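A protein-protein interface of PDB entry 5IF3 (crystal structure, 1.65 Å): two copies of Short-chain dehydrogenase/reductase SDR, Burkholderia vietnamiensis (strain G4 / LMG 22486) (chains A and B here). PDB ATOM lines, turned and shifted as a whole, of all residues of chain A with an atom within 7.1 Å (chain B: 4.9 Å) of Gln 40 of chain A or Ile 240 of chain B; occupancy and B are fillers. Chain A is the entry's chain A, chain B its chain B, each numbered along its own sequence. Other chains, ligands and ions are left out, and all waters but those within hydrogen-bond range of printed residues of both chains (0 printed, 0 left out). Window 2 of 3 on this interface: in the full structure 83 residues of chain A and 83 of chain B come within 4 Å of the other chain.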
ATOM      1  N   VAL A  18      21.821  -9.021   9.917  1.00  0.00           N
ATOM      2  CA  VAL A  18      20.410  -9.309  10.162  1.00  0.00           C
ATOM      3  C   VAL A  18      19.602  -8.121   9.673  1.00  0.00           C
ATOM      4  O   VAL A  18      19.927  -6.971   9.985  1.00  0.00           O
ATOM      5  CB  VAL A  18      20.148  -9.580  11.650  1.00  0.00           C
ATOM      6  CG1 VAL A  18      18.658  -9.823  11.891  1.00  0.00           C
ATOM      7  CG2 VAL A  18      20.960 -10.784  12.099  1.00  0.00           C
ATOM      8  N   SER A  32       6.934   1.459  15.772  1.00  0.00           N
ATOM      9  CA  SER A  32       7.639   0.896  16.922  1.00  0.00           C
ATOM     10  C   SER A  32       8.554  -0.247  16.500  1.00  0.00           C
ATOM     11  O   SER A  32       9.678  -0.367  17.004  1.00  0.00           O
ATOM     12  CB  SER A  32       6.640   0.405  17.972  1.00  0.00           C
ATOM     13  OG  SER A  32       5.907   1.484  18.514  1.00  0.00           O
ATOM     14  N   LEU A  33       8.085  -1.108  15.588  1.00  0.00           N
ATOM     15  CA  LEU A  33       8.927  -2.183  15.076  1.00  0.00           C
ATOM     16  C   LEU A  33      10.179  -1.634  14.404  1.00  0.00           C
ATOM     17  O   LEU A  33      11.303  -2.031  14.733  1.00  0.00           O
ATOM     18  CB  LEU A  33       8.134  -3.042  14.085  1.00  0.00           C
ATOM     19  CG  LEU A  33       7.099  -3.997  14.699  1.00  0.00           C
ATOM     20  CD1 LEU A  33       6.206  -4.601  13.611  1.00  0.00           C
ATOM     21  CD2 LEU A  33       7.794  -5.113  15.469  1.00  0.00           C
ATOM     22  N   ALA A  34       9.998  -0.707  13.463  1.00  0.00           N
ATOM     23  CA  ALA A  34      11.138  -0.172  12.721  1.00  0.00           C
ATOM     24  C   ALA A  34      12.130   0.513  13.656  1.00  0.00           C
ATOM     25  O   ALA A  34      13.345   0.301  13.548  1.00  0.00           O
ATOM     26  CB  ALA A  34      10.646   0.794  11.646  1.00  0.00           C
ATOM     27  N   GLU A  35      11.622   1.310  14.604  1.00  0.00           N
ATOM     28  CA  GLU A  35      12.491   2.024  15.537  1.00  0.00           C
ATOM     29  C   GLU A  35      13.318   1.056  16.374  1.00  0.00           C
ATOM     30  O   GLU A  35      14.529   1.241  16.541  1.00  0.00           O
ATOM     31  CB  GLU A  35      11.644   2.932  16.435  1.00  0.00           C
ATOM     32  CG  GLU A  35      10.966   4.059  15.682  1.00  0.00           C
ATOM     33  CD  GLU A  35       9.785   4.652  16.434  1.00  0.00           C
ATOM     34  OE1 GLU A  35       9.645   4.380  17.649  1.00  0.00           O
ATOM     35  OE2 GLU A  35       8.994   5.387  15.801  1.00  0.00           O
ATOM     36  N   GLN A  36      12.674   0.022  16.925  1.00  0.00           N
ATOM     37  CA  GLN A  36      13.380  -0.877  17.831  1.00  0.00           C
ATOM     38  C   GLN A  36      14.341  -1.784  17.078  1.00  0.00           C
ATOM     39  O   GLN A  36      15.420  -2.104  17.583  1.00  0.00           O
ATOM     40  CB  GLN A  36      12.377  -1.709  18.641  1.00  0.00           C
ATOM     41  CG  GLN A  36      11.575  -0.845  19.606  1.00  0.00           C
ATOM     42  CD  GLN A  36      10.617  -1.658  20.452  1.00  0.00           C
ATOM     43  OE1 GLN A  36      10.832  -2.845  20.684  1.00  0.00           O
ATOM     44  NE2 GLN A  36       9.560  -1.016  20.924  1.00  0.00           N
ATOM     45  N   LEU A  37      13.958  -2.234  15.881  1.00  0.00           N
ATOM     46  CA  LEU A  37      14.875  -3.039  15.077  1.00  0.00           C
ATOM     47  C   LEU A  37      16.163  -2.269  14.806  1.00  0.00           C
ATOM     48  O   LEU A  37      17.266  -2.791  15.001  1.00  0.00           O
ATOM     49  CB  LEU A  37      14.202  -3.448  13.769  1.00  0.00           C
ATOM     50  CG  LEU A  37      13.105  -4.502  13.949  1.00  0.00           C
ATOM     51  CD1 LEU A  37      12.185  -4.476  12.732  1.00  0.00           C
ATOM     52  CD2 LEU A  37      13.691  -5.885  14.190  1.00  0.00           C
ATOM     53  N   LEU A  38      16.039  -1.004  14.403  1.00  0.00           N
ATOM     54  CA  LEU A  38      17.225  -0.203  14.112  1.00  0.00           C
ATOM     55  C   LEU A  38      18.040   0.067  15.371  1.00  0.00           C
ATOM     56  O   LEU A  38      19.277   0.089  15.324  1.00  0.00           O
ATOM     57  CB  LEU A  38      16.810   1.100  13.429  1.00  0.00           C
ATOM     58  CG  LEU A  38      16.335   0.806  11.997  1.00  0.00           C
ATOM     59  CD1 LEU A  38      15.455   1.921  11.489  1.00  0.00           C
ATOM     60  CD2 LEU A  38      17.552   0.632  11.079  1.00  0.00           C
ATOM     61  N   GLN A  39      17.363   0.262  16.504  1.00  0.00           N
ATOM     62  CA  GLN A  39      18.072   0.414  17.773  1.00  0.00           C
ATOM     63  C   GLN A  39      18.963  -0.783  18.057  1.00  0.00           C
ATOM     64  O   GLN A  39      20.068  -0.629  18.601  1.00  0.00           O
ATOM     65  CB  GLN A  39      17.089   0.594  18.926  1.00  0.00           C
ATOM     66  CG  GLN A  39      16.403   1.916  18.953  1.00  0.00           C
ATOM     67  CD  GLN A  39      15.421   2.034  20.098  1.00  0.00           C
ATOM     68  OE1 GLN A  39      15.175   1.066  20.822  1.00  0.00           O
ATOM     69  NE2 GLN A  39      14.847   3.218  20.265  1.00  0.00           N
ATOM     70  N   GLN A  40      18.502  -1.988  17.693  1.00  0.00           N
ATOM     71  CA  GLN A  40      19.218  -3.233  17.939  1.00  0.00           C
ATOM     72  C   GLN A  40      20.109  -3.652  16.772  1.00  0.00           C
ATOM     73  O   GLN A  40      20.467  -4.831  16.671  1.00  0.00           O
ATOM     74  CB  GLN A  40      18.209  -4.332  18.296  1.00  0.00           C
ATOM     75  CG  GLN A  40      17.518  -4.019  19.608  1.00  0.00           C
ATOM     76  CD  GLN A  40      16.275  -4.869  19.846  1.00  0.00           C
ATOM     77  OE1 GLN A  40      15.368  -4.449  20.563  1.00  0.00           O
ATOM     78  NE2 GLN A  40      16.234  -6.060  19.252  1.00  0.00           N
ATOM     79  N   ASP A  41      20.461  -2.710  15.890  1.00  0.00           N
ATOM     80  CA  ASP A  41      21.405  -2.862  14.774  1.00  0.00           C
ATOM     81  C   ASP A  41      20.924  -3.897  13.763  1.00  0.00           C
ATOM     82  O   ASP A  41      21.701  -4.621  13.137  1.00  0.00           O
ATOM     83  CB  ASP A  41      22.822  -3.169  15.239  1.00  0.00           C
ATOM     84  CG  ASP A  41      23.856  -2.654  14.258  1.00  0.00           C
ATOM     85  OD1 ASP A  41      23.557  -1.671  13.525  1.00  0.00           O
ATOM     86  OD2 ASP A  41      24.951  -3.247  14.195  1.00  0.00           O
ATOM     87  N   ILE A  42      19.614  -3.893  13.529  1.00  0.00           N
ATOM     88  CA  ILE A  42      19.006  -4.639  12.421  1.00  0.00           C
ATOM     89  C   ILE A  42      18.566  -3.630  11.355  1.00  0.00           C
ATOM     90  O   ILE A  42      17.765  -2.729  11.636  1.00  0.00           O
ATOM     91  CB  ILE A  42      17.829  -5.495  12.911  1.00  0.00           C
ATOM     92  CG1 ILE A  42      18.329  -6.569  13.886  1.00  0.00           C
ATOM     93  CG2 ILE A  42      17.042  -6.088  11.726  1.00  0.00           C
ATOM     94  CD1 ILE A  42      17.213  -7.302  14.671  1.00  0.00           C
ATOM     95  N   ALA A  43      19.086  -3.777  10.133  1.00  0.00           N
ATOM     96  CA  ALA A  43      18.686  -2.898   9.037  1.00  0.00           C
ATOM     97  C   ALA A  43      17.208  -3.084   8.712  1.00  0.00           C
ATOM     98  O   ALA A  43      16.664  -4.186   8.810  1.00  0.00           O
ATOM     99  CB  ALA A  43      19.529  -3.179   7.782  1.00  0.00           C
ATOM    100  N   ARG A  62      20.933   2.834   7.390  1.00  0.00           N
ATOM    101  CA  ARG A  62      20.469   1.508   7.785  1.00  0.00           C
ATOM    102  C   ARG A  62      18.970   1.373   7.621  1.00  0.00           C
ATOM    103  O   ARG A  62      18.452   0.248   7.604  1.00  0.00           O
ATOM    104  CB  ARG A  62      20.877   1.237   9.227  1.00  0.00           C
ATOM    105  CG  ARG A  62      22.375   1.251   9.411  1.00  0.00           C
ATOM    106  CD  ARG A  62      22.743   1.918  10.721  1.00  0.00           C
ATOM    107  NE  ARG A  62      22.367   1.051  11.805  1.00  0.00           N
ATOM    108  CZ  ARG A  62      21.383   1.279  12.666  1.00  0.00           C
ATOM    109  NH1 ARG A  62      20.670   2.409  12.620  1.00  0.00           N
ATOM    110  NH2 ARG A  62      21.134   0.370  13.589  1.00  0.00           N
ATOM    111  N   LEU A  96      14.000 -10.852   8.382  1.00  0.00           N
ATOM    112  CA  LEU A  96      12.683 -10.910   9.004  1.00  0.00           C
ATOM    113  C   LEU A  96      11.705 -10.090   8.172  1.00  0.00           C
ATOM    114  O   LEU A  96      12.010  -8.957   7.793  1.00  0.00           O
ATOM    115  CB  LEU A  96      12.733 -10.351  10.429  1.00  0.00           C
ATOM    116  CG  LEU A  96      13.900 -10.680  11.361  1.00  0.00           C
ATOM    117  CD1 LEU A  96      13.795  -9.859  12.671  1.00  0.00           C
ATOM    118  CD2 LEU A  96      13.904 -12.160  11.668  1.00  0.00           C
ATOM    119  N   PHE A  98       8.066  -8.459   8.602  1.00  0.00           N
ATOM    120  CA  PHE A  98       6.939  -8.125   9.467  1.00  0.00           C
ATOM    121  C   PHE A  98       5.818  -7.618   8.571  1.00  0.00           C
ATOM    122  O   PHE A  98       5.849  -6.474   8.108  1.00  0.00           O
ATOM    123  CB  PHE A  98       7.331  -7.088  10.518  1.00  0.00           C
ATOM    124  CG  PHE A  98       8.326  -7.580  11.525  1.00  0.00           C
ATOM    125  CD1 PHE A  98       7.904  -8.142  12.725  1.00  0.00           C
ATOM    126  CD2 PHE A  98       9.692  -7.461  11.289  1.00  0.00           C
ATOM    127  CE1 PHE A  98       8.832  -8.597  13.655  1.00  0.00           C
ATOM    128  CE2 PHE A  98      10.628  -7.915  12.216  1.00  0.00           C
ATOM    129  CZ  PHE A  98      10.184  -8.481  13.416  1.00  0.00           C
ATOM    130  N   LEU A 149       6.702 -13.088   9.751  1.00  0.00           N
ATOM    131  CA  LEU A 149       5.776 -12.859  10.858  1.00  0.00           C
ATOM    132  C   LEU A 149       4.593 -12.080  10.301  1.00  0.00           C
ATOM    133  O   LEU A 149       4.723 -10.898   9.974  1.00  0.00           O
ATOM    134  CB  LEU A 149       6.475 -12.104  11.995  1.00  0.00           C
ATOM    135  CG  LEU A 149       5.706 -12.048  13.326  1.00  0.00           C
ATOM    136  CD1 LEU A 149       6.685 -11.782  14.476  1.00  0.00           C
ATOM    137  CD2 LEU A 149       4.599 -10.991  13.304  1.00  0.00           C
ATOM    138  N   ALA B 236       5.669  -4.247  19.989  1.00  0.00           N
ATOM    139  CA  ALA B 236       6.825  -4.410  19.111  1.00  0.00           C
ATOM    140  C   ALA B 236       7.956  -5.134  19.828  1.00  0.00           C
ATOM    141  O   ALA B 236       8.610  -6.012  19.253  1.00  0.00           O
ATOM    142  CB  ALA B 236       7.291  -3.042  18.621  1.00  0.00           C
ATOM    143  N   ARG B 237       8.182  -4.788  21.092  1.00  0.00           N
ATOM    144  CA  ARG B 237       9.230  -5.428  21.873  1.00  0.00           C
ATOM    145  C   ARG B 237       8.999  -6.929  21.947  1.00  0.00           C
ATOM    146  O   ARG B 237       9.911  -7.726  21.700  1.00  0.00           O
ATOM    147  CB  ARG B 237       9.268  -4.797  23.267  1.00  0.00           C
ATOM    148  CG  ARG B 237      10.295  -5.361  24.212  1.00  0.00           C
ATOM    149  CD  ARG B 237      10.433  -4.455  25.436  1.00  0.00           C
ATOM    150  NE  ARG B 237      10.607  -3.053  25.051  1.00  0.00           N
ATOM    151  CZ  ARG B 237       9.689  -2.102  25.218  1.00  0.00           C
ATOM    152  NH1 ARG B 237       8.524  -2.393  25.781  1.00  0.00           N
ATOM    153  NH2 ARG B 237       9.938  -0.856  24.830  1.00  0.00           N
ATOM    154  N   HIS B 238       7.758  -7.335  22.233  1.00  0.00           N
ATOM    155  CA  HIS B 238       7.458  -8.761  22.327  1.00  0.00           C
ATOM    156  C   HIS B 238       7.575  -9.449  20.972  1.00  0.00           C
ATOM    157  O   HIS B 238       8.096 -10.565  20.893  1.00  0.00           O
ATOM    158  CB  HIS B 238       6.062  -8.976  22.924  1.00  0.00           C
ATOM    159  CG  HIS B 238       5.957  -8.578  24.361  1.00  0.00           C
ATOM    160  ND1 HIS B 238       6.676  -9.201  25.357  1.00  0.00           N
ATOM    161  CD2 HIS B 238       5.219  -7.623  24.969  1.00  0.00           C
ATOM    162  CE1 HIS B 238       6.385  -8.644  26.519  1.00  0.00           C
ATOM    163  NE2 HIS B 238       5.502  -7.685  26.311  1.00  0.00           N
ATOM    164  N   LEU B 239       7.110  -8.797  19.897  1.00  0.00           N
ATOM    165  CA  LEU B 239       7.151  -9.419  18.571  1.00  0.00           C
ATOM    166  C   LEU B 239       8.584  -9.621  18.097  1.00  0.00           C
ATOM    167  O   LEU B 239       8.914 -10.659  17.509  1.00  0.00           O
ATOM    168  CB  LEU B 239       6.378  -8.564  17.571  1.00  0.00           C
ATOM    169  CG  LEU B 239       4.854  -8.512  17.667  1.00  0.00           C
ATOM    170  CD1 LEU B 239       4.336  -7.535  16.635  1.00  0.00           C
ATOM    171  CD2 LEU B 239       4.261  -9.885  17.452  1.00  0.00           C
ATOM    172  N   ILE B 240       9.452  -8.636  18.327  1.00  0.00           N
ATOM    173  CA  ILE B 240      10.823  -8.750  17.845  1.00  0.00           C
ATOM    174  C   ILE B 240      11.556  -9.849  18.598  1.00  0.00           C
ATOM    175  O   ILE B 240      12.260 -10.673  18.000  1.00  0.00           O
ATOM    176  CB  ILE B 240      11.546  -7.398  17.966  1.00  0.00           C
ATOM    177  CG1 ILE B 240      10.904  -6.368  17.030  1.00  0.00           C
ATOM    178  CG2 ILE B 240      13.025  -7.549  17.648  1.00  0.00           C
ATOM    179  CD1 ILE B 240      11.320  -4.910  17.325  1.00  0.00           C
ATOM    180  N   ARG B 241      11.402  -9.879  19.926  1.00  0.00           N
ATOM    181  CA  ARG B 241      12.034 -10.932  20.710  1.00  0.00           C
ATOM    182  C   ARG B 241      11.559 -12.300  20.239  1.00  0.00           C
ATOM    183  O   ARG B 241      12.368 -13.219  20.060  1.00  0.00           O
ATOM    184  CB  ARG B 241      11.734 -10.750  22.199  1.00  0.00           C
ATOM    185  CG  ARG B 241      12.453 -11.760  23.072  1.00  0.00           C
ATOM    186  CD  ARG B 241      12.003 -11.711  24.531  1.00  0.00           C
ATOM    187  NE  ARG B 241      11.909 -10.355  25.063  1.00  0.00           N
ATOM    188  CZ  ARG B 241      10.778  -9.794  25.486  1.00  0.00           C
ATOM    189  NH1 ARG B 241      10.786  -8.554  25.958  1.00  0.00           N
ATOM    190  NH2 ARG B 241       9.639 -10.477  25.444  1.00  0.00           N
ATOM    191  N   TYR B 242      10.252 -12.438  20.004  1.00  0.00           N
ATOM    192  CA  TYR B 242       9.717 -13.710  19.519  1.00  0.00           C
ATOM    193  C   TYR B 242      10.283 -14.059  18.158  1.00  0.00           C
ATOM    194  O   TYR B 242      10.699 -15.199  17.923  1.00  0.00           O
ATOM    195  CB  TYR B 242       8.197 -13.646  19.446  1.00  0.00           C
ATOM    196  CG  TYR B 242       7.564 -14.975  19.130  1.00  0.00           C
ATOM    197  CD1 TYR B 242       7.852 -16.086  19.896  1.00  0.00           C
ATOM    198  CD2 TYR B 242       6.665 -15.095  18.091  1.00  0.00           C
ATOM    199  CE1 TYR B 242       7.259 -17.299  19.637  1.00  0.00           C
ATOM    200  CE2 TYR B 242       6.051 -16.313  17.828  1.00  0.00           C
ATOM    201  CZ  TYR B 242       6.366 -17.405  18.601  1.00  0.00           C
ATOM    202  OH  TYR B 242       5.775 -18.626  18.364  1.00  0.00           O
ATOM    203  N   ALA B 243      10.310 -13.082  17.245  1.00  0.00           N
ATOM    204  CA  ALA B 243      10.777 -13.358  15.884  1.00  0.00           C
ATOM    205  C   ALA B 243      12.220 -13.834  15.869  1.00  0.00           C
ATOM    206  O   ALA B 243      12.590 -14.647  15.013  1.00  0.00           O
ATOM    207  CB  ALA B 243      10.626 -12.117  15.012  1.00  0.00           C
ATOM    208  N   LEU B 244      13.050 -13.344  16.791  1.00  0.00           N
ATOM    209  CA  LEU B 244      14.453 -13.731  16.832  1.00  0.00           C
ATOM    210  C   LEU B 244      14.711 -14.999  17.637  1.00  0.00           C
ATOM    211  O   LEU B 244      15.843 -15.503  17.618  1.00  0.00           O
ATOM    212  CB  LEU B 244      15.286 -12.579  17.407  1.00  0.00           C
ATOM    213  CG  LEU B 244      15.299 -11.342  16.508  1.00  0.00           C
ATOM    214  CD1 LEU B 244      15.869 -10.166  17.273  1.00  0.00           C
ATOM    215  CD2 LEU B 244      16.140 -11.600  15.261  1.00  0.00           C
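No position is printed for both chains. Of the 12 pairs that touch across the chains among the printed residues, none has its exchanged pair printed and touching as well.
Hydrophobic or aromatic side chains of chain A that line the printed part of chain B: Leu 33, Leu 37, Leu 96, Phe 98 and Leu 149. Of the 9 printed residues of chain B, 6 touch a printed residue of chain A. Among the printed residues, 12 pairs touch across the chains. Among the printed residues, no Asp or Glu carboxylate lies within 4 Å of a Lys or Arg side-chain nitrogen of the other chain.
Among the printed residues, pairs that only touch across the chains: Ser 32 of chain A with Ala 236 of chain B, Gln 36 of chain A with Ile 240 of chain B, Leu 33 of chain A with Ala 236 of chain B, Leu 33 of chain A with Ile 240 of chain B, Gln 36 of chain A with Ala 236 of chain B, Leu 37 of chain A with Ile 240 of chain B, Gln 40 of chain A with Ile 240 of chain B, Leu 96 of chain A with Leu 244 of chain B, Leu 149 of chain A with Leu 239 of chain B, Leu 149 of chain A with Ala 243 of chain B and Phe 98 of chain A with Ala 243 of chain B.
N of Ile 42 of chain A sits at hydrogen-bond distance from O of Leu 37 of chain A.
OE1 of Gln 36 of chain A sits close to N of Arg 237 of chain B.
Gln 40 of chain A touches one residue of chain B. Ile 240 of chain B touches just these residues of chain A: Leu 33 (3.7 Å), Gln 36 (3.6 Å), Leu 37 (3.8 Å) and Gln 40 (3.9 Å). Of the printed residues of chain A, Leu 244 of chain B touches Leu 96 (3.9 Å). Printed residues of chain B within 4 Å of Leu 96 of chain A: Leu 244. Of the printed residues of chain A, Ala 236 of chain B touches Ser 32, Leu 33 and Gln 36. Of the printed residues of chain B, Leu 33 of chain A touches Ala 236 and Ile 240. Of the printed residues of chain B, Leu 149 of chain A touches Leu 239 (3.9 Å) and Ala 243 (3.99 Å). The nearest residue of chain B that does not touch Gln 40 of chain A is Leu 244 of chain B (4.6 Å). The nearest printed residue of chain A that does not touch Ala 243 of chain B is Leu 96 of chain A (4.4 Å).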
